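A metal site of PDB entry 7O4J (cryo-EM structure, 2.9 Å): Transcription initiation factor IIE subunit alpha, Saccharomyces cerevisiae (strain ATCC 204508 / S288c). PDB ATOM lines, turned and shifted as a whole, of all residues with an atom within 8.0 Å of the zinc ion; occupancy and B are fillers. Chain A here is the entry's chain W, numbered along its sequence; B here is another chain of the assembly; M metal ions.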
ATOM      1  N   MET A 123      11.003  -2.902  -6.210  1.00  0.00           N
ATOM      2  CA  MET A 123      11.232  -1.824  -5.251  1.00  0.00           C
ATOM      3  C   MET A 123      11.751  -0.612  -6.009  1.00  0.00           C
ATOM      4  O   MET A 123      12.338  -0.733  -7.080  1.00  0.00           O
ATOM      5  CB  MET A 123      12.247  -2.236  -4.180  1.00  0.00           C
ATOM      6  CG  MET A 123      12.481  -1.191  -3.095  1.00  0.00           C
ATOM      7  SD  MET A 123      13.705  -1.715  -1.885  1.00  0.00           S
ATOM      8  CE  MET A 123      15.206  -1.630  -2.866  1.00  0.00           C
ATOM      9  N   CYS A 124      11.497   0.589  -5.442  1.00  0.00           N
ATOM     10  CA  CYS A 124      12.016   1.808  -6.038  1.00  0.00           C
ATOM     11  C   CYS A 124      13.285   2.237  -5.315  1.00  0.00           C
ATOM     12  O   CYS A 124      13.262   2.381  -4.076  1.00  0.00           O
ATOM     13  CB  CYS A 124      10.990   2.930  -5.969  1.00  0.00           C
ATOM     14  SG  CYS A 124      11.594   4.506  -6.635  1.00  0.00           S
ATOM     15  N   PRO A 125      14.403   2.442  -6.010  1.00  0.00           N
ATOM     16  CA  PRO A 125      15.652   2.780  -5.298  1.00  0.00           C
ATOM     17  C   PRO A 125      15.559   4.064  -4.499  1.00  0.00           C
ATOM     18  O   PRO A 125      16.216   4.185  -3.449  1.00  0.00           O
ATOM     19  CB  PRO A 125      16.679   2.881  -6.431  1.00  0.00           C
ATOM     20  CG  PRO A 125      15.885   3.183  -7.648  1.00  0.00           C
ATOM     21  CD  PRO A 125      14.577   2.467  -7.475  1.00  0.00           C
ATOM     22  N   ILE A 126      14.775   5.048  -4.959  1.00  0.00           N
ATOM     23  CA  ILE A 126      14.798   6.362  -4.340  1.00  0.00           C
ATOM     24  C   ILE A 126      13.883   6.411  -3.120  1.00  0.00           C
ATOM     25  O   ILE A 126      14.317   6.737  -2.015  1.00  0.00           O
ATOM     26  CB  ILE A 126      14.426   7.440  -5.371  1.00  0.00           C
ATOM     27  CG1 ILE A 126      15.462   7.466  -6.505  1.00  0.00           C
ATOM     28  CG2 ILE A 126      14.336   8.814  -4.708  1.00  0.00           C
ATOM     29  CD1 ILE A 126      15.065   8.323  -7.690  1.00  0.00           C
ATOM     30  N   CYS A 127      12.599   6.096  -3.309  1.00  0.00           N
ATOM     31  CA  CYS A 127      11.617   6.200  -2.228  1.00  0.00           C
ATOM     32  C   CYS A 127      11.499   4.933  -1.398  1.00  0.00           C
ATOM     33  O   CYS A 127      10.759   4.920  -0.415  1.00  0.00           O
ATOM     34  CB  CYS A 127      10.245   6.579  -2.796  1.00  0.00           C
ATOM     35  SG  CYS A 127       9.430   5.285  -3.763  1.00  0.00           S
ATOM     36  N   LEU A 128      12.214   3.871  -1.763  1.00  0.00           N
ATOM     37  CA  LEU A 128      12.235   2.635  -0.972  1.00  0.00           C
ATOM     38  C   LEU A 128      10.828   2.120  -0.705  1.00  0.00           C
ATOM     39  O   LEU A 128      10.466   1.765   0.417  1.00  0.00           O
ATOM     40  CB  LEU A 128      12.998   2.836   0.337  1.00  0.00           C
ATOM     41  CG  LEU A 128      14.455   3.318   0.243  1.00  0.00           C
ATOM     42  CD1 LEU A 128      15.180   3.017   1.538  1.00  0.00           C
ATOM     43  CD2 LEU A 128      15.175   2.678  -0.936  1.00  0.00           C
ATOM     44  N   THR A 129      10.012   2.090  -1.756  1.00  0.00           N
ATOM     45  CA  THR A 129       8.641   1.586  -1.684  1.00  0.00           C
ATOM     46  C   THR A 129       8.550   0.306  -2.501  1.00  0.00           C
ATOM     47  O   THR A 129       8.901   0.288  -3.681  1.00  0.00           O
ATOM     48  CB  THR A 129       7.640   2.612  -2.201  1.00  0.00           C
ATOM     49  OG1 THR A 129       7.956   2.966  -3.553  1.00  0.00           O
ATOM     50  CG2 THR A 129       7.639   3.860  -1.328  1.00  0.00           C
ATOM     51  N   TYR A 131       6.853  -2.698  -4.564  1.00  0.00           N
ATOM     52  CA  TYR A 131       5.731  -2.942  -5.463  1.00  0.00           C
ATOM     53  C   TYR A 131       5.645  -4.424  -5.764  1.00  0.00           C
ATOM     54  O   TYR A 131       6.658  -5.072  -6.058  1.00  0.00           O
ATOM     55  CB  TYR A 131       5.887  -2.153  -6.762  1.00  0.00           C
ATOM     56  CG  TYR A 131       5.664  -0.668  -6.625  1.00  0.00           C
ATOM     57  CD1 TYR A 131       4.465  -0.165  -6.135  1.00  0.00           C
ATOM     58  CD2 TYR A 131       6.653   0.234  -6.994  1.00  0.00           C
ATOM     59  CE1 TYR A 131       4.262   1.196  -6.012  1.00  0.00           C
ATOM     60  CE2 TYR A 131       6.455   1.592  -6.864  1.00  0.00           C
ATOM     61  CZ  TYR A 131       5.259   2.073  -6.373  1.00  0.00           C
ATOM     62  OH  TYR A 131       5.064   3.435  -6.256  1.00  0.00           O
ATOM     63  N   LEU A 148       7.894   2.044 -14.091  1.00  0.00           N
ATOM     64  CA  LEU A 148       8.151   3.367 -13.537  1.00  0.00           C
ATOM     65  C   LEU A 148       7.491   3.522 -12.174  1.00  0.00           C
ATOM     66  O   LEU A 148       6.375   3.032 -11.943  1.00  0.00           O
ATOM     67  CB  LEU A 148       7.644   4.449 -14.480  1.00  0.00           C
ATOM     68  CG  LEU A 148       8.593   4.929 -15.579  1.00  0.00           C
ATOM     69  CD1 LEU A 148       9.839   5.566 -14.988  1.00  0.00           C
ATOM     70  CD2 LEU A 148       8.972   3.762 -16.489  1.00  0.00           C
ATOM     71  N   CYS A 149       8.190   4.184 -11.255  1.00  0.00           N
ATOM     72  CA  CYS A 149       7.613   4.491  -9.955  1.00  0.00           C
ATOM     73  C   CYS A 149       6.537   5.562 -10.094  1.00  0.00           C
ATOM     74  O   CYS A 149       6.498   6.328 -11.059  1.00  0.00           O
ATOM     75  CB  CYS A 149       8.706   4.946  -8.984  1.00  0.00           C
ATOM     76  SG  CYS A 149       8.089   5.586  -7.407  1.00  0.00           S
ATOM     77  N   SER A 150       5.645   5.596  -9.110  1.00  0.00           N
ATOM     78  CA  SER A 150       4.567   6.575  -9.075  1.00  0.00           C
ATOM     79  C   SER A 150       5.011   7.902  -8.462  1.00  0.00           C
ATOM     80  O   SER A 150       4.776   8.960  -9.050  1.00  0.00           O
ATOM     81  CB  SER A 150       3.365   6.023  -8.305  1.00  0.00           C
ATOM     82  OG  SER A 150       2.206   6.794  -8.536  1.00  0.00           O
ATOM     83  N   LEU A 151       5.632   7.854  -7.285  1.00  0.00           N
ATOM     84  CA  LEU A 151       6.073   9.086  -6.644  1.00  0.00           C
ATOM     85  C   LEU A 151       7.265   9.701  -7.379  1.00  0.00           C
ATOM     86  O   LEU A 151       7.281  10.909  -7.643  1.00  0.00           O
ATOM     87  CB  LEU A 151       6.440   8.808  -5.190  1.00  0.00           C
ATOM     88  CG  LEU A 151       6.548  10.023  -4.254  1.00  0.00           C
ATOM     89  CD1 LEU A 151       6.345   9.592  -2.808  1.00  0.00           C
ATOM     90  CD2 LEU A 151       7.884  10.735  -4.423  1.00  0.00           C
ATOM     91  N   CYS A 152       8.252   8.883  -7.726  1.00  0.00           N
ATOM     92  CA  CYS A 152       9.503   9.371  -8.296  1.00  0.00           C
ATOM     93  C   CYS A 152       9.534   9.356  -9.816  1.00  0.00           C
ATOM     94  O   CYS A 152      10.346  10.076 -10.407  1.00  0.00           O
ATOM     95  CB  CYS A 152      10.676   8.538  -7.772  1.00  0.00           C
ATOM     96  SG  CYS A 152      10.585   8.136  -6.015  1.00  0.00           S
ATOM     97  N   ASP A 153       8.677   8.570 -10.457  1.00  0.00           N
ATOM     98  CA  ASP A 153       8.699   8.415 -11.911  1.00  0.00           C
ATOM     99  C   ASP A 153      10.080   7.955 -12.361  1.00  0.00           C
ATOM    100  O   ASP A 153      10.710   8.540 -13.243  1.00  0.00           O
ATOM    101  CB  ASP A 153       8.290   9.708 -12.600  1.00  0.00           C
ATOM    102  CG  ASP A 153       8.145   9.545 -14.103  1.00  0.00           C
ATOM    103  OD1 ASP A 153       8.206   8.388 -14.587  1.00  0.00           O
ATOM    104  OD2 ASP A 153       7.976  10.560 -14.799  1.00  0.00           O
ATOM    105  N   GLU A 154      10.544   6.878 -11.727  1.00  0.00           N
ATOM    106  CA  GLU A 154      11.872   6.324 -11.953  1.00  0.00           C
ATOM    107  C   GLU A 154      11.758   4.827 -12.173  1.00  0.00           C
ATOM    108  O   GLU A 154      10.854   4.189 -11.610  1.00  0.00           O
ATOM    109  CB  GLU A 154      12.800   6.611 -10.758  1.00  0.00           C
ATOM    110  CG  GLU A 154      14.285   6.547 -11.064  1.00  0.00           C
ATOM    111  CD  GLU A 154      14.880   5.181 -10.797  1.00  0.00           C
ATOM    112  OE1 GLU A 154      14.435   4.509  -9.839  1.00  0.00           O
ATOM    113  OE2 GLU A 154      15.810   4.771 -11.534  1.00  0.00           O
ATOM    114  N   PRO A 155      12.633   4.231 -12.975  1.00  0.00           N
ATOM    115  CA  PRO A 155      12.563   2.783 -13.194  1.00  0.00           C
ATOM    116  C   PRO A 155      12.696   1.998 -11.899  1.00  0.00           C
ATOM    117  O   PRO A 155      13.425   2.379 -10.976  1.00  0.00           O
ATOM    118  CB  PRO A 155      13.743   2.501 -14.129  1.00  0.00           C
ATOM    119  CG  PRO A 155      13.921   3.764 -14.874  1.00  0.00           C
ATOM    120  CD  PRO A 155      13.578   4.871 -13.923  1.00  0.00           C
ATOM    121  N   LEU A 156      11.963   0.885 -11.823  1.00  0.00           N
ATOM    122  CA  LEU A 156      11.966   0.013 -10.665  1.00  0.00           C
ATOM    123  C   LEU A 156      13.107  -1.000 -10.774  1.00  0.00           C
ATOM    124  O   LEU A 156      13.582  -1.314 -11.870  1.00  0.00           O
ATOM    125  CB  LEU A 156      10.631  -0.728 -10.535  1.00  0.00           C
ATOM    126  CG  LEU A 156       9.470  -0.035  -9.808  1.00  0.00           C
ATOM    127  CD1 LEU A 156       9.816   0.264  -8.358  1.00  0.00           C
ATOM    128  CD2 LEU A 156       9.039   1.229 -10.533  1.00  0.00           C
ATOM    129  N   PRO B  16      12.137  11.225  -0.986  1.00  0.00           N
ATOM    130  CA  PRO B  16      11.154  11.614  -1.998  1.00  0.00           C
ATOM    131  C   PRO B  16      11.168  13.122  -2.240  1.00  0.00           C
ATOM    132  O   PRO B  16      11.373  13.909  -1.321  1.00  0.00           O
ATOM    133  CB  PRO B  16       9.824  11.140  -1.416  1.00  0.00           C
ATOM    134  CG  PRO B  16      10.178  10.136  -0.379  1.00  0.00           C
ATOM    135  CD  PRO B  16      11.507  10.558   0.164  1.00  0.00           C
HETATM  136 ZN    ZN M   1       9.884   5.920  -5.957  1.00  0.00          ZN
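The zinc ion is bound by the side-chain sulfur of Cys 124 (2.3 Å), the side-chain sulfur of Cys 152 (2.3 Å), the side-chain sulfur of Cys 127 (2.3 Å) and the side-chain sulfur of Cys 149 (2.3 Å).
Of the 18 residues printed, 4 come within 4 Å of the zinc ion.
SG of Cys 124 sits close to N of Ile 126. SG of Cys 127 lies close to OG1 of Thr 129. N of Leu 151 lies close to SG of Cys 149. The backbone carbonyl oxygen (O) of Thr 129 is in hydrogen-bond range of the backbone NH (N) of Cys 124. The backbone NH (N) of Cys 149 lies within hydrogen-bond range of the backbone carbonyl oxygen (O) of Glu 154 (2.7 Å).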
